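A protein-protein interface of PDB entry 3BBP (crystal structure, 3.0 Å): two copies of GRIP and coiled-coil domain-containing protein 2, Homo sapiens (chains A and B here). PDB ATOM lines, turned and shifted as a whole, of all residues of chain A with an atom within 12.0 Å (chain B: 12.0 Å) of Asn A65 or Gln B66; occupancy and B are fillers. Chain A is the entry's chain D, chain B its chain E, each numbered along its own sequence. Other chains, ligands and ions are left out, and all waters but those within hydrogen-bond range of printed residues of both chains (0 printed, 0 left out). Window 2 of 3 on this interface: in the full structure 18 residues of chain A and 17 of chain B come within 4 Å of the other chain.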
ATOM      1  N   LEU A  55      22.955 -16.137 -11.912  1.00  0.00           N
ATOM      2  CA  LEU A  55      21.686 -15.424 -11.829  1.00  0.00           C
ATOM      3  C   LEU A  55      21.864 -13.945 -12.171  1.00  0.00           C
ATOM      4  O   LEU A  55      21.105 -13.393 -12.966  1.00  0.00           O
ATOM      5  CB  LEU A  55      21.081 -15.572 -10.429  1.00  0.00           C
ATOM      6  CG  LEU A  55      20.608 -16.970 -10.019  1.00  0.00           C
ATOM      7  CD1 LEU A  55      20.290 -17.033  -8.524  1.00  0.00           C
ATOM      8  CD2 LEU A  55      19.405 -17.400 -10.857  1.00  0.00           C
ATOM      9  N   LYS A  56      22.873 -13.315 -11.576  1.00  0.00           N
ATOM     10  CA  LYS A  56      23.117 -11.892 -11.776  1.00  0.00           C
ATOM     11  C   LYS A  56      23.302 -11.544 -13.246  1.00  0.00           C
ATOM     12  O   LYS A  56      22.734 -10.567 -13.734  1.00  0.00           O
ATOM     13  CB  LYS A  56      24.327 -11.422 -10.959  1.00  0.00           C
ATOM     14  CG  LYS A  56      24.049 -11.266  -9.465  1.00  0.00           C
ATOM     15  CD  LYS A  56      25.297 -10.855  -8.704  1.00  0.00           C
ATOM     16  CE  LYS A  56      25.057 -10.841  -7.203  1.00  0.00           C
ATOM     17  NZ  LYS A  56      26.345 -10.817  -6.460  1.00  0.00           N
ATOM     18  N   SER A  57      24.101 -12.337 -13.951  1.00  0.00           N
ATOM     19  CA  SER A  57      24.349 -12.089 -15.369  1.00  0.00           C
ATOM     20  C   SER A  57      23.091 -12.358 -16.193  1.00  0.00           C
ATOM     21  O   SER A  57      22.855 -11.712 -17.212  1.00  0.00           O
ATOM     22  CB  SER A  57      25.522 -12.932 -15.874  1.00  0.00           C
ATOM     23  OG  SER A  57      25.272 -14.311 -15.689  1.00  0.00           O
ATOM     24  N   GLU A  58      22.283 -13.310 -15.740  1.00  0.00           N
ATOM     25  CA  GLU A  58      20.990 -13.578 -16.357  1.00  0.00           C
ATOM     26  C   GLU A  58      20.073 -12.363 -16.226  1.00  0.00           C
ATOM     27  O   GLU A  58      19.327 -12.034 -17.145  1.00  0.00           O
ATOM     28  CB  GLU A  58      20.338 -14.814 -15.729  1.00  0.00           C
ATOM     29  CG  GLU A  58      19.017 -15.226 -16.366  1.00  0.00           C
ATOM     30  CD  GLU A  58      19.135 -15.509 -17.857  1.00  0.00           C
ATOM     31  OE1 GLU A  58      20.275 -15.617 -18.367  1.00  0.00           O
ATOM     32  OE2 GLU A  58      18.079 -15.625 -18.519  1.00  0.00           O
ATOM     33  N   ILE A  59      20.135 -11.696 -15.078  1.00  0.00           N
ATOM     34  CA  ILE A  59      19.386 -10.459 -14.880  1.00  0.00           C
ATOM     35  C   ILE A  59      19.886  -9.377 -15.838  1.00  0.00           C
ATOM     36  O   ILE A  59      19.097  -8.742 -16.537  1.00  0.00           O
ATOM     37  CB  ILE A  59      19.481  -9.959 -13.423  1.00  0.00           C
ATOM     38  CG1 ILE A  59      18.779 -10.942 -12.483  1.00  0.00           C
ATOM     39  CG2 ILE A  59      18.876  -8.566 -13.286  1.00  0.00           C
ATOM     40  CD1 ILE A  59      18.845 -10.549 -11.022  1.00  0.00           C
ATOM     41  N   ARG A  60      21.200  -9.176 -15.870  1.00  0.00           N
ATOM     42  CA  ARG A  60      21.803  -8.192 -16.760  1.00  0.00           C
ATOM     43  C   ARG A  60      21.446  -8.475 -18.218  1.00  0.00           C
ATOM     44  O   ARG A  60      21.262  -7.551 -19.013  1.00  0.00           O
ATOM     45  CB  ARG A  60      23.322  -8.178 -16.592  1.00  0.00           C
ATOM     46  CG  ARG A  60      23.812  -7.892 -15.176  1.00  0.00           C
ATOM     47  CD  ARG A  60      25.321  -7.678 -15.154  1.00  0.00           C
ATOM     48  NE  ARG A  60      25.919  -7.969 -13.852  1.00  0.00           N
ATOM     49  CZ  ARG A  60      26.019  -7.090 -12.865  1.00  0.00           C
ATOM     50  NH1 ARG A  60      25.549  -5.859 -13.029  1.00  0.00           N
ATOM     51  NH2 ARG A  60      26.582  -7.441 -11.714  1.00  0.00           N
ATOM     52  N   ARG A  61      21.354  -9.756 -18.564  1.00  0.00           N
ATOM     53  CA  ARG A  61      20.989 -10.165 -19.917  1.00  0.00           C
ATOM     54  C   ARG A  61      19.560  -9.769 -20.272  1.00  0.00           C
ATOM     55  O   ARG A  61      19.304  -9.242 -21.348  1.00  0.00           O
ATOM     56  CB  ARG A  61      21.151 -11.674 -20.092  1.00  0.00           C
ATOM     57  CG  ARG A  61      20.928 -12.144 -21.518  1.00  0.00           C
ATOM     58  CD  ARG A  61      20.968 -13.660 -21.621  1.00  0.00           C
ATOM     59  NE  ARG A  61      19.727 -14.281 -21.166  1.00  0.00           N
ATOM     60  CZ  ARG A  61      18.622 -14.367 -21.902  1.00  0.00           C
ATOM     61  NH1 ARG A  61      18.603 -13.865 -23.133  1.00  0.00           N
ATOM     62  NH2 ARG A  61      17.537 -14.950 -21.407  1.00  0.00           N
ATOM     63  N   LEU A  62      18.630 -10.033 -19.364  1.00  0.00           N
ATOM     64  CA  LEU A  62      17.233  -9.685 -19.588  1.00  0.00           C
ATOM     65  C   LEU A  62      17.041  -8.174 -19.719  1.00  0.00           C
ATOM     66  O   LEU A  62      16.243  -7.710 -20.534  1.00  0.00           O
ATOM     67  CB  LEU A  62      16.361 -10.234 -18.456  1.00  0.00           C
ATOM     68  CG  LEU A  62      16.219 -11.755 -18.402  1.00  0.00           C
ATOM     69  CD1 LEU A  62      15.521 -12.185 -17.119  1.00  0.00           C
ATOM     70  CD2 LEU A  62      15.469 -12.256 -19.624  1.00  0.00           C
ATOM     71  N   GLU A  63      17.778  -7.411 -18.917  1.00  0.00           N
ATOM     72  CA  GLU A  63      17.660  -5.954 -18.920  1.00  0.00           C
ATOM     73  C   GLU A  63      18.129  -5.331 -20.237  1.00  0.00           C
ATOM     74  O   GLU A  63      17.633  -4.281 -20.647  1.00  0.00           O
ATOM     75  CB  GLU A  63      18.422  -5.351 -17.738  1.00  0.00           C
ATOM     76  CG  GLU A  63      17.780  -5.624 -16.389  1.00  0.00           C
ATOM     77  CD  GLU A  63      18.543  -5.004 -15.231  1.00  0.00           C
ATOM     78  OE1 GLU A  63      19.770  -4.794 -15.362  1.00  0.00           O
ATOM     79  OE2 GLU A  63      17.910  -4.736 -14.186  1.00  0.00           O
ATOM     80  N   ARG A  64      19.083  -5.983 -20.895  1.00  0.00           N
ATOM     81  CA  ARG A  64      19.591  -5.508 -22.175  1.00  0.00           C
ATOM     82  C   ARG A  64      18.557  -5.664 -23.293  1.00  0.00           C
ATOM     83  O   ARG A  64      18.331  -4.739 -24.078  1.00  0.00           O
ATOM     84  CB  ARG A  64      20.889  -6.239 -22.537  1.00  0.00           C
ATOM     85  CG  ARG A  64      22.063  -5.903 -21.626  1.00  0.00           C
ATOM     86  CD  ARG A  64      23.384  -6.344 -22.248  1.00  0.00           C
ATOM     87  NE  ARG A  64      23.423  -7.784 -22.502  1.00  0.00           N
ATOM     88  CZ  ARG A  64      23.916  -8.681 -21.649  1.00  0.00           C
ATOM     89  NH1 ARG A  64      24.414  -8.290 -20.482  1.00  0.00           N
ATOM     90  NH2 ARG A  64      23.908  -9.968 -21.962  1.00  0.00           N
ATOM     91  N   ASN A  65      17.933  -6.837 -23.358  1.00  0.00           N
ATOM     92  CA  ASN A  65      16.903  -7.113 -24.354  1.00  0.00           C
ATOM     93  C   ASN A  65      15.548  -6.533 -23.945  1.00  0.00           C
ATOM     94  O   ASN A  65      14.497  -7.093 -24.265  1.00  0.00           O
ATOM     95  CB  ASN A  65      16.771  -8.620 -24.602  1.00  0.00           C
ATOM     96  CG  ASN A  65      18.113  -9.302 -24.803  1.00  0.00           C
ATOM     97  OD1 ASN A  65      18.935  -9.365 -23.892  1.00  0.00           O
ATOM     98  ND2 ASN A  65      18.333  -9.828 -25.998  1.00  0.00           N
ATOM     99  N   GLN A  66      15.582  -5.410 -23.233  1.00  0.00           N
ATOM    100  CA  GLN A  66      14.362  -4.750 -22.783  1.00  0.00           C
ATOM    101  C   GLN A  66      13.995  -3.599 -23.718  1.00  0.00           C
ATOM    102  O   GLN A  66      14.870  -2.890 -24.223  1.00  0.00           O
ATOM    103  CB  GLN A  66      14.539  -4.228 -21.356  1.00  0.00           C
ATOM    104  CG  GLN A  66      13.240  -3.887 -20.646  1.00  0.00           C
ATOM    105  CD  GLN A  66      12.511  -5.116 -20.140  1.00  0.00           C
ATOM    106  OE1 GLN A  66      11.348  -5.044 -19.743  1.00  0.00           O
ATOM    107  NE2 GLN A  66      13.194  -6.254 -20.151  1.00  0.00           N
ATOM    108  N   SER B  57      13.289 -14.146  -8.211  1.00  0.00           N
ATOM    109  CA  SER B  57      12.010 -13.474  -8.422  1.00  0.00           C
ATOM    110  C   SER B  57      12.185 -12.227  -9.289  1.00  0.00           C
ATOM    111  O   SER B  57      11.292 -11.858 -10.057  1.00  0.00           O
ATOM    112  CB  SER B  57      11.362 -13.110  -7.087  1.00  0.00           C
ATOM    113  OG  SER B  57      12.204 -12.253  -6.344  1.00  0.00           O
ATOM    114  N   GLU B  58      13.343 -11.586  -9.167  1.00  0.00           N
ATOM    115  CA  GLU B  58      13.698 -10.468 -10.034  1.00  0.00           C
ATOM    116  C   GLU B  58      13.801 -10.919 -11.492  1.00  0.00           C
ATOM    117  O   GLU B  58      13.415 -10.193 -12.409  1.00  0.00           O
ATOM    118  CB  GLU B  58      15.015  -9.831  -9.578  1.00  0.00           C
ATOM    119  CG  GLU B  58      15.418  -8.591 -10.365  1.00  0.00           C
ATOM    120  CD  GLU B  58      14.368  -7.486 -10.329  1.00  0.00           C
ATOM    121  OE1 GLU B  58      13.425  -7.566  -9.506  1.00  0.00           O
ATOM    122  OE2 GLU B  58      14.491  -6.530 -11.128  1.00  0.00           O
ATOM    123  N   ILE B  59      14.320 -12.124 -11.702  1.00  0.00           N
ATOM    124  CA  ILE B  59      14.370 -12.711 -13.038  1.00  0.00           C
ATOM    125  C   ILE B  59      12.961 -12.970 -13.559  1.00  0.00           C
ATOM    126  O   ILE B  59      12.618 -12.559 -14.668  1.00  0.00           O
ATOM    127  CB  ILE B  59      15.189 -14.020 -13.063  1.00  0.00           C
ATOM    128  CG1 ILE B  59      16.664 -13.721 -12.785  1.00  0.00           C
ATOM    129  CG2 ILE B  59      15.044 -14.723 -14.400  1.00  0.00           C
ATOM    130  CD1 ILE B  59      17.545 -14.945 -12.759  1.00  0.00           C
ATOM    131  N   ARG B  60      12.146 -13.640 -12.749  1.00  0.00           N
ATOM    132  CA  ARG B  60      10.758 -13.921 -13.109  1.00  0.00           C
ATOM    133  C   ARG B  60       9.989 -12.638 -13.410  1.00  0.00           C
ATOM    134  O   ARG B  60       9.129 -12.617 -14.291  1.00  0.00           O
ATOM    135  CB  ARG B  60      10.050 -14.696 -11.992  1.00  0.00           C
ATOM    136  CG  ARG B  60      10.719 -16.003 -11.573  1.00  0.00           C
ATOM    137  CD  ARG B  60       9.838 -16.793 -10.614  1.00  0.00           C
ATOM    138  NE  ARG B  60      10.593 -17.720  -9.772  1.00  0.00           N
ATOM    139  CZ  ARG B  60      10.916 -18.960 -10.123  1.00  0.00           C
ATOM    140  NH1 ARG B  60      10.554 -19.424 -11.314  1.00  0.00           N
ATOM    141  NH2 ARG B  60      11.602 -19.732  -9.285  1.00  0.00           N
ATOM    142  N   ARG B  61      10.299 -11.574 -12.673  1.00  0.00           N
ATOM    143  CA  ARG B  61       9.668 -10.274 -12.887  1.00  0.00           C
ATOM    144  C   ARG B  61      10.012  -9.685 -14.252  1.00  0.00           C
ATOM    145  O   ARG B  61       9.138  -9.192 -14.963  1.00  0.00           O
ATOM    146  CB  ARG B  61      10.083  -9.284 -11.804  1.00  0.00           C
ATOM    147  CG  ARG B  61       9.349  -7.955 -11.901  1.00  0.00           C
ATOM    148  CD  ARG B  61       9.844  -6.955 -10.874  1.00  0.00           C
ATOM    149  NE  ARG B  61      11.103  -6.345 -11.284  1.00  0.00           N
ATOM    150  CZ  ARG B  61      11.188  -5.348 -12.155  1.00  0.00           C
ATOM    151  NH1 ARG B  61      10.085  -4.861 -12.708  1.00  0.00           N
ATOM    152  NH2 ARG B  61      12.371  -4.841 -12.479  1.00  0.00           N
ATOM    153  N   LEU B  62      11.291  -9.729 -14.607  1.00  0.00           N
ATOM    154  CA  LEU B  62      11.744  -9.201 -15.888  1.00  0.00           C
ATOM    155  C   LEU B  62      11.136  -9.967 -17.057  1.00  0.00           C
ATOM    156  O   LEU B  62      10.775  -9.375 -18.074  1.00  0.00           O
ATOM    157  CB  LEU B  62      13.272  -9.224 -15.969  1.00  0.00           C
ATOM    158  CG  LEU B  62      14.011  -8.241 -15.053  1.00  0.00           C
ATOM    159  CD1 LEU B  62      15.509  -8.507 -15.060  1.00  0.00           C
ATOM    160  CD2 LEU B  62      13.720  -6.803 -15.458  1.00  0.00           C
ATOM    161  N   GLU B  63      11.017 -11.282 -16.903  1.00  0.00           N
ATOM    162  CA  GLU B  63      10.474 -12.134 -17.961  1.00  0.00           C
ATOM    163  C   GLU B  63       8.998 -11.855 -18.243  1.00  0.00           C
ATOM    164  O   GLU B  63       8.527 -12.028 -19.369  1.00  0.00           O
ATOM    165  CB  GLU B  63      10.690 -13.615 -17.626  1.00  0.00           C
ATOM    166  CG  GLU B  63      12.146 -14.053 -17.686  1.00  0.00           C
ATOM    167  CD  GLU B  63      12.337 -15.525 -17.367  1.00  0.00           C
ATOM    168  OE1 GLU B  63      11.492 -16.101 -16.640  1.00  0.00           O
ATOM    169  OE2 GLU B  63      13.341 -16.100 -17.844  1.00  0.00           O
ATOM    170  N   ARG B  64       8.269 -11.424 -17.220  1.00  0.00           N
ATOM    171  CA  ARG B  64       6.855 -11.106 -17.372  1.00  0.00           C
ATOM    172  C   ARG B  64       6.651  -9.836 -18.198  1.00  0.00           C
ATOM    173  O   ARG B  64       5.819  -9.803 -19.105  1.00  0.00           O
ATOM    174  CB  ARG B  64       6.188 -10.968 -16.004  1.00  0.00           C
ATOM    175  CG  ARG B  64       6.108 -12.269 -15.220  1.00  0.00           C
ATOM    176  CD  ARG B  64       5.118 -12.157 -14.069  1.00  0.00           C
ATOM    177  NE  ARG B  64       5.493 -11.113 -13.122  1.00  0.00           N
ATOM    178  CZ  ARG B  64       6.208 -11.331 -12.022  1.00  0.00           C
ATOM    179  NH1 ARG B  64       6.615 -12.557 -11.729  1.00  0.00           N
ATOM    180  NH2 ARG B  64       6.512 -10.327 -11.214  1.00  0.00           N
ATOM    181  N   ASN B  65       7.417  -8.796 -17.880  1.00  0.00           N
ATOM    182  CA  ASN B  65       7.346  -7.537 -18.616  1.00  0.00           C
ATOM    183  C   ASN B  65       8.139  -7.586 -19.921  1.00  0.00           C
ATOM    184  O   ASN B  65       8.696  -6.578 -20.360  1.00  0.00           O
ATOM    185  CB  ASN B  65       7.843  -6.381 -17.748  1.00  0.00           C
ATOM    186  CG  ASN B  65       7.248  -6.401 -16.357  1.00  0.00           C
ATOM    187  OD1 ASN B  65       7.504  -7.312 -15.574  1.00  0.00           O
ATOM    188  ND2 ASN B  65       6.456  -5.388 -16.039  1.00  0.00           N
ATOM    189  N   GLN B  66       8.184  -8.764 -20.534  1.00  0.00           N
ATOM    190  CA  GLN B  66       8.907  -8.951 -21.785  1.00  0.00           C
ATOM    191  C   GLN B  66       7.946  -8.900 -22.969  1.00  0.00           C
ATOM    192  O   GLN B  66       6.811  -9.381 -22.884  1.00  0.00           O
ATOM    193  CB  GLN B  66       9.652 -10.288 -21.773  1.00  0.00           C
ATOM    194  CG  GLN B  66      10.735 -10.413 -22.830  1.00  0.00           C
ATOM    195  CD  GLN B  66      12.000  -9.666 -22.460  1.00  0.00           C
ATOM    196  OE1 GLN B  66      12.889  -9.478 -23.290  1.00  0.00           O
ATOM    197  NE2 GLN B  66      12.091  -9.238 -21.207  1.00  0.00           N
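Ile B59 touches its own counterpart, Ile A59. Leu B62 touches its own counterpart, Leu A62. Leu A62 touches Glu B63, and with the chains exchanged Glu A63 touches Leu B62. Asn A65 touches Gln B66, and with the chains exchanged Gln A66 touches Asn B65. Of the 11 pairs that touch across the chains among the printed residues, 9 have their exchanged pair printed and touching as well.
Of the printed residues of chain B, Glu A58 touches Ile B59. Of the printed residues of chain B, Ile A59 touches Ile B59 (3.5 Å) and Leu B62 (3.8 Å). No residue of chain B comes within 4 Å of Arg A61. Of the printed residues of chain B, Glu A63 touches Leu B62 (3.9 Å). No residue of chain B comes within 4 Å of Arg A64. Of the printed residues of chain B, Asn A65 touches Gln B66. Gln A66 touches two residues of chain B. Of the printed residues of chain A, Ile B59 touches Leu A55 (3.6 Å), Glu A58 (3.9 Å), Ile A59 (3.5 Å) and Leu A62 (3.7 Å). Arg B60 touches none of the printed residues of chain A. Of the printed residues of chain A, Leu B62 touches Ile A59, Leu A62 and Glu A63. Printed residues of chain A within 4 Å of Glu B63: Leu A62 (3.9 Å). Of the printed residues of chain A, Asn B65 touches Gln A66 (3.1 Å). Gln B66 touches two residues of chain A. The nearest residue of chain B that does not touch Asn A65 is Asn B65 (7.0 Å). The nearest residue of chain A that does not touch Gln B66 is Leu A62 (4.5 Å).
The backbone carbonyl oxygen (O) of Arg B61 sits close to the side-chain amide oxygen (OD1) of Asn B65 (2.6 Å). The side-chain carboxylate (OE2) of Glu A58 lies within salt-bridge range of the guanidinium group (NH2) of Arg A61, at 3.0 Å. The backbone carbonyl oxygen (O) of Leu A62 is in hydrogen-bond range of the side-chain amide nitrogen (NE2) of Gln A66, 3.4 Å away. The backbone carbonyl oxygen (O) of Leu B62 is in hydrogen-bond range of the side-chain amide nitrogen (NE2) of Gln B66, at 3.4 Å. The backbone carbonyl oxygen (O) of Arg A61 sits close to the side-chain amide oxygen (OD1) of Asn A65, at 2.6 Å.
Of the 10 printed residues of chain B, 5 touch a printed residue of chain A. Of the 12 printed residues of chain A, 7 touch a printed residue of chain B. Hydrophobic or aromatic side chains of chain A that line the printed part of chain B: Leu A55, Ile A59 and Leu A62. Among the printed residues, no Asp or Glu carboxylate lies within 4 Å of a Lys or Arg side-chain nitrogen of the other chain.
The side-chain amide oxygen of Gln B66 sits close to the backbone carbonyl oxygen of Asn A65 (3.0 Å). The side-chain amide nitrogen (NE2) of Gln B66 sits close to the side-chain amide nitrogen (NE2) of Gln A66, at 3.4 Å. O of Asn B65 sits close to OE1 of Gln A66 (3.1 Å).
Leu A55 touches Ile B59 (CD2 to CD1, 3.6 Å). CG of Glu A58 touches CD1 of Ile B59 (3.9 Å). CG1 of Ile A59 touches CG1 of Ile B59 (3.5 Å). Leu B62 touches Ile A59 (CD1 to CG2, 3.8 Å). Leu A62 touches Ile B59. Leu B62 touches Leu A62 (CB to CD1, 3.9 Å). Leu A62 touches Glu B63. Glu A63 touches Leu B62 (CG to CD1, 3.9 Å).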
